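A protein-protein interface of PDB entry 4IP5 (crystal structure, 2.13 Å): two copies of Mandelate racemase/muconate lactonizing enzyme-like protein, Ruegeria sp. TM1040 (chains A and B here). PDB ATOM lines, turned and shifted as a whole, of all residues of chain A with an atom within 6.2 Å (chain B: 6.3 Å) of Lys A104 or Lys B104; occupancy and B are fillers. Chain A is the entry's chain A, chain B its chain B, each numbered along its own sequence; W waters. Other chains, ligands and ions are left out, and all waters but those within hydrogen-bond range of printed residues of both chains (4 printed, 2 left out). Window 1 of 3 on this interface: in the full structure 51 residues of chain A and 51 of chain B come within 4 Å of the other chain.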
ATOM      1  N   ILE A 100     -33.037  22.192  -1.013  1.00  0.00           N
ATOM      2  CA  ILE A 100     -32.763  22.919  -2.251  1.00  0.00           C
ATOM      3  C   ILE A 100     -31.824  22.107  -3.153  1.00  0.00           C
ATOM      4  O   ILE A 100     -31.731  22.356  -4.354  1.00  0.00           O
ATOM      5  CB  ILE A 100     -32.169  24.304  -1.913  1.00  0.00           C
ATOM      6  CG1 ILE A 100     -33.041  24.993  -0.854  1.00  0.00           C
ATOM      7  CG2 ILE A 100     -32.010  25.176  -3.155  1.00  0.00           C
ATOM      8  CD1 ILE A 100     -34.529  25.071  -1.220  1.00  0.00           C
ATOM      9  N   GLY A 101     -31.120  21.147  -2.554  1.00  0.00           N
ATOM     10  CA  GLY A 101     -30.312  20.182  -3.285  1.00  0.00           C
ATOM     11  C   GLY A 101     -31.014  18.825  -3.321  1.00  0.00           C
ATOM     12  O   GLY A 101     -31.977  18.649  -4.069  1.00  0.00           O
ATOM     13  N   PRO A 102     -30.544  17.856  -2.509  1.00  0.00           N
ATOM     14  CA  PRO A 102     -29.379  17.963  -1.620  1.00  0.00           C
ATOM     15  C   PRO A 102     -28.079  17.720  -2.369  1.00  0.00           C
ATOM     16  O   PRO A 102     -28.053  16.860  -3.249  1.00  0.00           O
ATOM     17  CB  PRO A 102     -29.593  16.818  -0.608  1.00  0.00           C
ATOM     18  CG  PRO A 102     -31.010  16.244  -0.905  1.00  0.00           C
ATOM     19  CD  PRO A 102     -31.249  16.569  -2.341  1.00  0.00           C
ATOM     20  N   ASP A 103     -27.024  18.445  -1.999  1.00  0.00           N
ATOM     21  CA  ASP A 103     -25.697  18.271  -2.597  1.00  0.00           C
ATOM     22  C   ASP A 103     -25.741  18.284  -4.129  1.00  0.00           C
ATOM     23  O   ASP A 103     -25.171  17.421  -4.787  1.00  0.00           O
ATOM     24  CB  ASP A 103     -25.025  16.989  -2.083  1.00  0.00           C
ATOM     25  CG  ASP A 103     -24.690  17.051  -0.590  1.00  0.00           C
ATOM     26  OD1 ASP A 103     -24.911  18.116   0.034  1.00  0.00           O
ATOM     27  OD2 ASP A 103     -24.196  16.036  -0.043  1.00  0.00           O
ATOM     28  N   LYS A 104     -26.435  19.265  -4.688  1.00  0.00           N
ATOM     29  CA  LYS A 104     -26.498  19.428  -6.138  1.00  0.00           C
ATOM     30  C   LYS A 104     -27.001  20.822  -6.456  1.00  0.00           C
ATOM     31  O   LYS A 104     -27.562  21.499  -5.587  1.00  0.00           O
ATOM     32  CB  LYS A 104     -27.427  18.385  -6.763  1.00  0.00           C
ATOM     33  CG  LYS A 104     -28.896  18.666  -6.515  1.00  0.00           C
ATOM     34  CD  LYS A 104     -29.773  17.457  -6.874  1.00  0.00           C
ATOM     35  CE  LYS A 104     -29.513  16.264  -5.988  1.00  0.00           C
ATOM     36  NZ  LYS A 104     -30.553  15.227  -6.232  1.00  0.00           N
ATOM     37  N   GLY A 105     -26.808  21.255  -7.696  1.00  0.00           N
ATOM     38  CA  GLY A 105     -27.304  22.555  -8.121  1.00  0.00           C
ATOM     39  C   GLY A 105     -26.678  23.729  -7.383  1.00  0.00           C
ATOM     40  O   GLY A 105     -25.575  23.630  -6.828  1.00  0.00           O
ATOM     41  N   ALA A 106     -27.410  24.836  -7.361  1.00  0.00           N
ATOM     42  CA  ALA A 106     -26.949  26.081  -6.765  1.00  0.00           C
ATOM     43  C   ALA A 106     -26.406  25.943  -5.341  1.00  0.00           C
ATOM     44  O   ALA A 106     -25.369  26.521  -5.010  1.00  0.00           O
ATOM     45  CB  ALA A 106     -28.060  27.111  -6.803  1.00  0.00           C
ATOM     46  N   ILE A 107     -27.106  25.198  -4.493  1.00  0.00           N
ATOM     47  CA  ILE A 107     -26.727  25.150  -3.084  1.00  0.00           C
ATOM     48  C   ILE A 107     -25.359  24.477  -2.915  1.00  0.00           C
ATOM     49  O   ILE A 107     -24.603  24.817  -2.013  1.00  0.00           O
ATOM     50  CB  ILE A 107     -27.811  24.469  -2.189  1.00  0.00           C
ATOM     51  CG1 ILE A 107     -27.573  24.775  -0.703  1.00  0.00           C
ATOM     52  CG2 ILE A 107     -27.853  22.956  -2.422  1.00  0.00           C
ATOM     53  CD1 ILE A 107     -27.599  26.273  -0.356  1.00  0.00           C
ATOM     54  N   HIS A 108     -25.030  23.550  -3.809  1.00  0.00           N
ATOM     55  CA  HIS A 108     -23.786  22.802  -3.676  1.00  0.00           C
ATOM     56  C   HIS A 108     -22.604  23.510  -4.350  1.00  0.00           C
ATOM     57  O   HIS A 108     -21.488  23.469  -3.832  1.00  0.00           O
ATOM     58  CB  HIS A 108     -23.951  21.372  -4.195  1.00  0.00           C
ATOM     59  CG  HIS A 108     -23.156  20.363  -3.430  1.00  0.00           C
ATOM     60  ND1 HIS A 108     -22.941  20.466  -2.072  1.00  0.00           N
ATOM     61  CD2 HIS A 108     -22.531  19.228  -3.825  1.00  0.00           C
ATOM     62  CE1 HIS A 108     -22.209  19.441  -1.664  1.00  0.00           C
ATOM     63  NE2 HIS A 108     -21.950  18.674  -2.708  1.00  0.00           N
ATOM     64  N   LEU A 109     -22.853  24.147  -5.496  1.00  0.00           N
ATOM     65  CA  LEU A 109     -21.889  25.075  -6.089  1.00  0.00           C
ATOM     66  C   LEU A 109     -21.473  26.074  -5.011  1.00  0.00           C
ATOM     67  O   LEU A 109     -20.284  26.321  -4.795  1.00  0.00           O
ATOM     68  CB  LEU A 109     -22.522  25.817  -7.275  1.00  0.00           C
ATOM     69  CG  LEU A 109     -22.803  25.003  -8.540  1.00  0.00           C
ATOM     70  CD1 LEU A 109     -23.817  25.714  -9.453  1.00  0.00           C
ATOM     71  CD2 LEU A 109     -21.511  24.759  -9.292  1.00  0.00           C
ATOM     72  N   PRO A 277     -24.822  14.601 -17.721  1.00  0.00           N
ATOM     73  CA  PRO A 277     -23.875  14.296 -16.641  1.00  0.00           C
ATOM     74  C   PRO A 277     -24.497  13.431 -15.540  1.00  0.00           C
ATOM     75  O   PRO A 277     -23.781  12.997 -14.642  1.00  0.00           O
ATOM     76  CB  PRO A 277     -23.517  15.676 -16.095  1.00  0.00           C
ATOM     77  CG  PRO A 277     -24.709  16.510 -16.373  1.00  0.00           C
ATOM     78  CD  PRO A 277     -25.304  15.990 -17.666  1.00  0.00           C
ATOM     79  N   ASP A 278     -25.805  13.196 -15.618  1.00  0.00           N
ATOM     80  CA  ASP A 278     -26.524  12.370 -14.650  1.00  0.00           C
ATOM     81  C   ASP A 278     -26.694  10.935 -15.146  1.00  0.00           C
ATOM     82  O   ASP A 278     -27.138  10.065 -14.398  1.00  0.00           O
ATOM     83  CB  ASP A 278     -27.940  12.931 -14.414  1.00  0.00           C
ATOM     84  CG  ASP A 278     -27.937  14.351 -13.875  1.00  0.00           C
ATOM     85  OD1 ASP A 278     -26.898  14.799 -13.329  1.00  0.00           O
ATOM     86  OD2 ASP A 278     -28.986  15.019 -13.991  1.00  0.00           O
ATOM     87  N   MET A 300     -19.533  18.354 -14.433  1.00  0.00           N
ATOM     88  CA  MET A 300     -20.817  18.708 -13.829  1.00  0.00           C
ATOM     89  C   MET A 300     -21.405  17.604 -12.935  1.00  0.00           C
ATOM     90  O   MET A 300     -22.576  17.685 -12.536  1.00  0.00           O
ATOM     91  CB  MET A 300     -21.844  19.076 -14.906  1.00  0.00           C
ATOM     92  CG  MET A 300     -21.634  20.429 -15.535  1.00  0.00           C
ATOM     93  SD  MET A 300     -23.209  20.996 -16.216  1.00  0.00           S
ATOM     94  CE  MET A 300     -22.621  22.356 -17.220  1.00  0.00           C
ATOM     95  N   CYS A 301     -20.619  16.569 -12.638  1.00  0.00           N
ATOM     96  CA  CYS A 301     -21.128  15.476 -11.810  1.00  0.00           C
ATOM     97  C   CYS A 301     -21.391  16.057 -10.428  1.00  0.00           C
ATOM     98  O   CYS A 301     -20.511  16.679  -9.841  1.00  0.00           O
ATOM     99  CB  CYS A 301     -20.139  14.310 -11.748  1.00  0.00           C
ATOM    100  SG  CYS A 301     -20.724  12.890 -10.761  1.00  0.00           S
ATOM    101  N   GLN A 302     -22.607  15.878  -9.921  1.00  0.00           N
ATOM    102  CA  GLN A 302     -23.094  16.721  -8.823  1.00  0.00           C
ATOM    103  C   GLN A 302     -22.441  16.487  -7.462  1.00  0.00           C
ATOM    104  O   GLN A 302     -22.271  17.429  -6.689  1.00  0.00           O
ATOM    105  CB  GLN A 302     -24.620  16.630  -8.700  1.00  0.00           C
ATOM    106  CG  GLN A 302     -25.133  15.232  -8.443  1.00  0.00           C
ATOM    107  CD  GLN A 302     -26.590  15.055  -8.899  1.00  0.00           C
ATOM    108  OE1 GLN A 302     -26.965  15.497  -9.979  1.00  0.00           O
ATOM    109  NE2 GLN A 302     -27.405  14.407  -8.071  1.00  0.00           N
ATOM    110  N   ASN A 303     -22.073  15.246  -7.172  1.00  0.00           N
ATOM    111  CA  ASN A 303     -21.552  14.909  -5.844  1.00  0.00           C
ATOM    112  C   ASN A 303     -20.909  13.529  -5.808  1.00  0.00           C
ATOM    113  O   ASN A 303     -20.876  12.831  -6.821  1.00  0.00           O
ATOM    114  CB  ASN A 303     -22.669  15.005  -4.798  1.00  0.00           C
ATOM    115  CG  ASN A 303     -23.836  14.073  -5.105  1.00  0.00           C
ATOM    116  OD1 ASN A 303     -23.637  12.960  -5.588  1.00  0.00           O
ATOM    117  ND2 ASN A 303     -25.064  14.533  -4.826  1.00  0.00           N
ATOM    118  N   ARG A 325     -17.694  22.454  -8.357  1.00  0.00           N
ATOM    119  CA  ARG A 325     -19.035  21.967  -8.689  1.00  0.00           C
ATOM    120  C   ARG A 325     -19.613  21.277  -7.457  1.00  0.00           C
ATOM    121  O   ARG A 325     -20.788  21.445  -7.142  1.00  0.00           O
ATOM    122  CB  ARG A 325     -18.988  20.999  -9.878  1.00  0.00           C
ATOM    123  CG  ARG A 325     -20.241  20.136 -10.110  1.00  0.00           C
ATOM    124  CD  ARG A 325     -21.495  20.944 -10.489  1.00  0.00           C
ATOM    125  NE  ARG A 325     -21.295  21.836 -11.638  1.00  0.00           N
ATOM    126  CZ  ARG A 325     -22.280  22.499 -12.242  1.00  0.00           C
ATOM    127  NH1 ARG A 325     -23.535  22.363 -11.814  1.00  0.00           N
ATOM    128  NH2 ARG A 325     -22.020  23.291 -13.280  1.00  0.00           N
ATOM    129  N   ILE B 100     -26.261  26.052 -13.779  1.00  0.00           N
ATOM    130  CA  ILE B 100     -26.643  26.091 -12.366  1.00  0.00           C
ATOM    131  C   ILE B 100     -27.282  24.748 -11.966  1.00  0.00           C
ATOM    132  O   ILE B 100     -27.401  24.419 -10.779  1.00  0.00           O
ATOM    133  CB  ILE B 100     -27.606  27.282 -12.105  1.00  0.00           C
ATOM    134  CG1 ILE B 100     -27.055  28.550 -12.763  1.00  0.00           C
ATOM    135  CG2 ILE B 100     -27.817  27.518 -10.621  1.00  0.00           C
ATOM    136  CD1 ILE B 100     -25.674  28.972 -12.246  1.00  0.00           C
ATOM    137  N   GLY B 101     -27.678  23.977 -12.976  1.00  0.00           N
ATOM    138  CA  GLY B 101     -28.237  22.646 -12.785  1.00  0.00           C
ATOM    139  C   GLY B 101     -27.279  21.587 -13.302  1.00  0.00           C
ATOM    140  O   GLY B 101     -26.295  21.287 -12.637  1.00  0.00           O
ATOM    141  N   PRO B 102     -27.563  21.001 -14.485  1.00  0.00           N
ATOM    142  CA  PRO B 102     -28.786  21.176 -15.281  1.00  0.00           C
ATOM    143  C   PRO B 102     -29.944  20.327 -14.749  1.00  0.00           C
ATOM    144  O   PRO B 102     -29.729  19.206 -14.274  1.00  0.00           O
ATOM    145  CB  PRO B 102     -28.376  20.686 -16.686  1.00  0.00           C
ATOM    146  CG  PRO B 102     -26.841  20.520 -16.634  1.00  0.00           C
ATOM    147  CD  PRO B 102     -26.558  20.200 -15.202  1.00  0.00           C
ATOM    148  N   ASP B 103     -31.159  20.861 -14.836  1.00  0.00           N
ATOM    149  CA  ASP B 103     -32.343  20.107 -14.451  1.00  0.00           C
ATOM    150  C   ASP B 103     -32.180  19.490 -13.050  1.00  0.00           C
ATOM    151  O   ASP B 103     -32.448  18.311 -12.845  1.00  0.00           O
ATOM    152  CB  ASP B 103     -32.633  19.020 -15.497  1.00  0.00           C
ATOM    153  CG  ASP B 103     -33.119  19.598 -16.830  1.00  0.00           C
ATOM    154  OD1 ASP B 103     -33.186  20.836 -16.958  1.00  0.00           O
ATOM    155  OD2 ASP B 103     -33.427  18.821 -17.756  1.00  0.00           O
ATOM    156  N   LYS B 104     -31.707  20.288 -12.099  1.00  0.00           N
ATOM    157  CA  LYS B 104     -31.582  19.826 -10.720  1.00  0.00           C
ATOM    158  C   LYS B 104     -31.419  21.012  -9.784  1.00  0.00           C
ATOM    159  O   LYS B 104     -30.982  22.094 -10.195  1.00  0.00           O
ATOM    160  CB  LYS B 104     -30.373  18.892 -10.555  1.00  0.00           C
ATOM    161  CG  LYS B 104     -29.029  19.624 -10.627  1.00  0.00           C
ATOM    162  CD  LYS B 104     -27.848  18.650 -10.691  1.00  0.00           C
ATOM    163  CE  LYS B 104     -27.839  17.817 -11.976  1.00  0.00           C
ATOM    164  NZ  LYS B 104     -26.551  17.045 -12.113  1.00  0.00           N
ATOM    165  N   GLY B 105     -31.744  20.800  -8.515  1.00  0.00           N
ATOM    166  CA  GLY B 105     -31.577  21.836  -7.517  1.00  0.00           C
ATOM    167  C   GLY B 105     -32.492  23.028  -7.750  1.00  0.00           C
ATOM    168  O   GLY B 105     -33.557  22.907  -8.365  1.00  0.00           O
ATOM    169  N   ALA B 106     -32.050  24.186  -7.276  1.00  0.00           N
ATOM    170  CA  ALA B 106     -32.854  25.403  -7.284  1.00  0.00           C
ATOM    171  C   ALA B 106     -33.403  25.771  -8.657  1.00  0.00           C
ATOM    172  O   ALA B 106     -34.563  26.167  -8.775  1.00  0.00           O
ATOM    173  CB  ALA B 106     -32.056  26.567  -6.708  1.00  0.00           C
ATOM    174  N   ILE B 107     -32.576  25.650  -9.693  1.00  0.00           N
ATOM    175  CA  ILE B 107     -33.013  26.059 -11.024  1.00  0.00           C
ATOM    176  C   ILE B 107     -34.128  25.149 -11.552  1.00  0.00           C
ATOM    177  O   ILE B 107     -34.970  25.589 -12.329  1.00  0.00           O
ATOM    178  CB  ILE B 107     -31.838  26.145 -12.041  1.00  0.00           C
ATOM    179  CG1 ILE B 107     -32.263  26.917 -13.294  1.00  0.00           C
ATOM    180  CG2 ILE B 107     -31.343  24.758 -12.431  1.00  0.00           C
ATOM    181  CD1 ILE B 107     -32.635  28.382 -13.037  1.00  0.00           C
ATOM    182  N   HIS B 108     -34.154  23.887 -11.127  1.00  0.00           N
ATOM    183  CA  HIS B 108     -35.193  22.979 -11.627  1.00  0.00           C
ATOM    184  C   HIS B 108     -36.453  23.056 -10.765  1.00  0.00           C
ATOM    185  O   HIS B 108     -37.569  22.940 -11.273  1.00  0.00           O
ATOM    186  CB  HIS B 108     -34.688  21.533 -11.759  1.00  0.00           C
ATOM    187  CG  HIS B 108     -35.280  20.802 -12.927  1.00  0.00           C
ATOM    188  ND1 HIS B 108     -35.533  21.417 -14.136  1.00  0.00           N
ATOM    189  CD2 HIS B 108     -35.682  19.517 -13.069  1.00  0.00           C
ATOM    190  CE1 HIS B 108     -36.052  20.537 -14.976  1.00  0.00           C
ATOM    191  NE2 HIS B 108     -36.152  19.375 -14.353  1.00  0.00           N
ATOM    192  N   LEU B 109     -36.273  23.269  -9.463  1.00  0.00           N
ATOM    193  CA  LEU B 109     -37.413  23.563  -8.592  1.00  0.00           C
ATOM    194  C   LEU B 109     -38.183  24.743  -9.166  1.00  0.00           C
ATOM    195  O   LEU B 109     -39.405  24.703  -9.281  1.00  0.00           O
ATOM    196  CB  LEU B 109     -36.935  23.878  -7.166  1.00  0.00           C
ATOM    197  CG  LEU B 109     -36.381  22.666  -6.414  1.00  0.00           C
ATOM    198  CD1 LEU B 109     -35.460  23.087  -5.258  1.00  0.00           C
ATOM    199  CD2 LEU B 109     -37.542  21.849  -5.901  1.00  0.00           C
ATOM    200  N   PRO B 277     -31.374  10.234  -2.432  1.00  0.00           N
ATOM    201  CA  PRO B 277     -32.268  10.175  -3.600  1.00  0.00           C
ATOM    202  C   PRO B 277     -31.512  10.087  -4.927  1.00  0.00           C
ATOM    203  O   PRO B 277     -32.151   9.969  -5.981  1.00  0.00           O
ATOM    204  CB  PRO B 277     -33.044  11.496  -3.514  1.00  0.00           C
ATOM    205  CG  PRO B 277     -32.092  12.437  -2.797  1.00  0.00           C
ATOM    206  CD  PRO B 277     -31.316  11.581  -1.830  1.00  0.00           C
ATOM    207  N   ASP B 278     -30.182  10.146  -4.868  1.00  0.00           N
ATOM    208  CA  ASP B 278     -29.329  10.034  -6.051  1.00  0.00           C
ATOM    209  C   ASP B 278     -28.808   8.624  -6.235  1.00  0.00           C
ATOM    210  O   ASP B 278     -28.216   8.296  -7.269  1.00  0.00           O
ATOM    211  CB  ASP B 278     -28.110  10.950  -5.906  1.00  0.00           C
ATOM    212  CG  ASP B 278     -28.490  12.396  -5.782  1.00  0.00           C
ATOM    213  OD1 ASP B 278     -29.640  12.740  -6.155  1.00  0.00           O
ATOM    214  OD2 ASP B 278     -27.639  13.183  -5.315  1.00  0.00           O
ATOM    215  N   MET B 300     -37.624  13.544  -4.127  1.00  0.00           N
ATOM    216  CA  MET B 300     -36.517  14.444  -4.457  1.00  0.00           C
ATOM    217  C   MET B 300     -35.730  13.984  -5.683  1.00  0.00           C
ATOM    218  O   MET B 300     -34.656  14.527  -5.976  1.00  0.00           O
ATOM    219  CB  MET B 300     -35.546  14.576  -3.284  1.00  0.00           C
ATOM    220  CG  MET B 300     -36.056  15.387  -2.122  1.00  0.00           C
ATOM    221  SD  MET B 300     -34.661  15.995  -1.168  1.00  0.00           S
ATOM    222  CE  MET B 300     -35.491  16.787   0.196  1.00  0.00           C
ATOM    223  N   CYS B 301     -36.230  12.971  -6.386  1.00  0.00           N
ATOM    224  CA  CYS B 301     -35.524  12.512  -7.573  1.00  0.00           C
ATOM    225  C   CYS B 301     -35.501  13.692  -8.549  1.00  0.00           C
ATOM    226  O   CYS B 301     -36.544  14.270  -8.854  1.00  0.00           O
ATOM    227  CB  CYS B 301     -36.195  11.292  -8.179  1.00  0.00           C
ATOM    228  SG  CYS B 301     -35.289  10.665  -9.612  1.00  0.00           S
ATOM    229  N   GLN B 302     -34.308  14.084  -8.985  1.00  0.00           N
ATOM    230  CA  GLN B 302     -34.117  15.414  -9.564  1.00  0.00           C
ATOM    231  C   GLN B 302     -34.745  15.620 -10.944  1.00  0.00           C
ATOM    232  O   GLN B 302     -35.201  16.726 -11.257  1.00  0.00           O
ATOM    233  CB  GLN B 302     -32.624  15.790  -9.595  1.00  0.00           C
ATOM    234  CG  GLN B 302     -31.776  14.957 -10.569  1.00  0.00           C
ATOM    235  CD  GLN B 302     -30.319  14.900 -10.146  1.00  0.00           C
ATOM    236  OE1 GLN B 302     -30.008  14.834  -8.953  1.00  0.00           O
ATOM    237  NE2 GLN B 302     -29.418  14.928 -11.118  1.00  0.00           N
ATOM    238  N   ASN B 303     -34.763  14.576 -11.769  1.00  0.00           N
ATOM    239  CA  ASN B 303     -35.233  14.732 -13.146  1.00  0.00           C
ATOM    240  C   ASN B 303     -35.524  13.400 -13.818  1.00  0.00           C
ATOM    241  O   ASN B 303     -35.337  12.344 -13.209  1.00  0.00           O
ATOM    242  CB  ASN B 303     -34.218  15.547 -13.967  1.00  0.00           C
ATOM    243  CG  ASN B 303     -32.868  14.877 -14.052  1.00  0.00           C
ATOM    244  OD1 ASN B 303     -32.768  13.646 -14.077  1.00  0.00           O
ATOM    245  ND2 ASN B 303     -31.805  15.689 -14.099  1.00  0.00           N
ATOM    246  N   ARG B 325     -40.770  19.200  -7.938  1.00  0.00           N
ATOM    247  CA  ARG B 325     -39.343  18.967  -7.750  1.00  0.00           C
ATOM    248  C   ARG B 325     -38.636  19.054  -9.103  1.00  0.00           C
ATOM    249  O   ARG B 325     -37.553  19.623  -9.220  1.00  0.00           O
ATOM    250  CB  ARG B 325     -39.111  17.587  -7.115  1.00  0.00           C
ATOM    251  CG  ARG B 325     -37.672  17.069  -7.151  1.00  0.00           C
ATOM    252  CD  ARG B 325     -36.666  17.987  -6.424  1.00  0.00           C
ATOM    253  NE  ARG B 325     -36.997  18.190  -5.012  1.00  0.00           N
ATOM    254  CZ  ARG B 325     -36.186  18.761  -4.122  1.00  0.00           C
ATOM    255  NH1 ARG B 325     -34.967  19.183  -4.490  1.00  0.00           N
ATOM    256  NH2 ARG B 325     -36.589  18.913  -2.861  1.00  0.00           N
HETATM  257  O   HOH W   1     -24.751  19.070 -11.932  1.00  0.00           O
HETATM  258  O   HOH W   2     -33.100  16.564  -5.659  1.00  0.00           O
HETATM  259  O   HOH W   3     -28.739  14.271  -3.271  1.00  0.00           O
HETATM  260  O   HOH W   4     -28.396  17.000 -15.468  1.00  0.00           O
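N of Ala B106 lies within hydrogen-bond range of O of Ile A100. The backbone carbonyl oxygen of Gly A101 sits at hydrogen-bond distance from the guanidinium group of Arg B325. NZ of Lys A104 is in salt-bridge range of OD1 of Asp B278 (2.7 Å). OE1 of Gln B302 sits at hydrogen-bond distance from NZ of Lys A104, 2.8 Å away. O of Ile B100 sits at hydrogen-bond distance from N of Ala A106, at 3.4 Å. The side-chain carboxylate (OD1) of Asp A278 lies within salt-bridge range of the side-chain amino group (NZ) of Lys B104 (2.6 Å). The side-chain amide nitrogen (NE2) of Gln B302 is in hydrogen-bond range of the side-chain carboxylate (OD2) of Asp A278 (2.9 Å). OD2 of Asp A278 is in hydrogen-bond range of ND2 of Asn B303. The side-chain amide oxygen (OE1) of Gln A302 lies within hydrogen-bond range of the side-chain amino group (NZ) of Lys B104, 2.7 Å away. NE2 of Gln A302 sits at hydrogen-bond distance from OD2 of Asp B278 (3.0 Å). The side-chain amide nitrogen of Gln B302 is in hydrogen-bond range of the side-chain amide oxygen of Gln A302, 2.8 Å away. The side-chain amide nitrogen (ND2) of Asn A303 lies within hydrogen-bond range of the side-chain carboxylate (OD2) of Asp B278 (2.9 Å). The guanidinium group (NH1) of Arg A325 lies within hydrogen-bond range of the backbone carbonyl oxygen (O) of Gly B101.
The backbone carbonyl oxygen (O) of Asp A103 sits at hydrogen-bond distance from the side-chain amide nitrogen (ND2) of Asn A303 (2.9 Å). OD1 of Asp A278 sits close to OE1 of Gln A302 (3.4 Å). O of Asp B103 lies within hydrogen-bond range of ND2 of Asn B303.
Ile A100 touches Gly B105 (O to CA, 3.2 Å). Ile A100 touches Leu B109 (O to CD1, 3.9 Å). Pro A102 touches Met B300 (CD to SD, 3.7 Å). CD of Lys B104 touches CB of Lys A104 (3.96 Å). CA of Gly A105 touches O of Ile B100 (3.2 Å). CD of Pro B102 touches SD of Met A300 (3.6 Å).
Of the printed residues of chain B, Gly A101 touches Arg B325 (3.1 Å). Lys A104 touches just these residues of chain B: Lys B104 (3.96 Å), Asp B278 (2.7 Å) and Gln B302 (2.8 Å). Of the printed residues of chain B, Ala A106 touches Ile B100. Of the printed residues of chain B, Gln A302 touches Lys B104 (2.7 Å), Asp B278 (3.0 Å) and Gln B302 (2.8 Å). Of the printed residues of chain A, Ile B100 touches Gly A105 (3.2 Å) and Ala A106 (3.4 Å). Of the printed residues of chain A, Lys B104 touches Lys A104, Asp A278 and Gln A302. His B108 touches none of the printed residues of chain A. Of the printed residues of chain A, Leu B109 touches Ile A100. Cys B301 touches none of the printed residues of chain A.
Of the 17 printed residues of chain B, 12 touch a printed residue of chain A. Hydrophobic or aromatic side chains of chain B that line the printed part of chain A: Ile B100, Pro B102, Ala B106, Leu B109 and Met B300. Hydrophobic or aromatic side chains of chain A that line the printed part of chain B: Ile A100, Pro A102, Ala A106 and Met A300. Among the printed residues, Asp or Glu carboxylates within 4 Å of a Lys or Arg side-chain nitrogen of the other chain: Lys A104 with Asp B278 and Asp A278 with Lys B104.
Ile A100 touches Gly B105, and with the chains exchanged Gly A105 touches Ile B100. Pro A102 touches Met B300, and with the chains exchanged Met A300 touches Pro B102. Lys A104 touches Asp B278, and with the chains exchanged Asp A278 touches Lys B104. Lys A104 touches Gln B302, and with the chains exchanged Gln A302 touches Lys B104. Positions printed for both chains: 100, 101, 102, 103, 104, 105, 106, 107, 108, 109, 277, 278, 300, 301, 302, 303 and 325. Of the 19 pairs that touch across the chains among the printed residues, 18 have their exchanged pair printed and touching as well.
Water W4 bridges OD2 of Asp A278 (2.5 Å) and O of Pro B102 (2.8 Å). Water W3 lies within hydrogen-bond range of the side-chain carboxylate (OD2) of Asp B278 (2.6 Å) and the backbone carbonyl oxygen (O) of Pro A102 (2.7 Å). Water W2 lies within hydrogen-bond range of the backbone carbonyl oxygen of Met B300, the backbone carbonyl oxygen of Gly A101, the side-chain amino group of Lys A104 and the guanidinium group of Arg B325. Water W1 lies within hydrogen-bond range of O of Met A300 (2.6 Å), NZ of Lys B104 (2.7 Å) and O of Gly B101 (2.8 Å).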
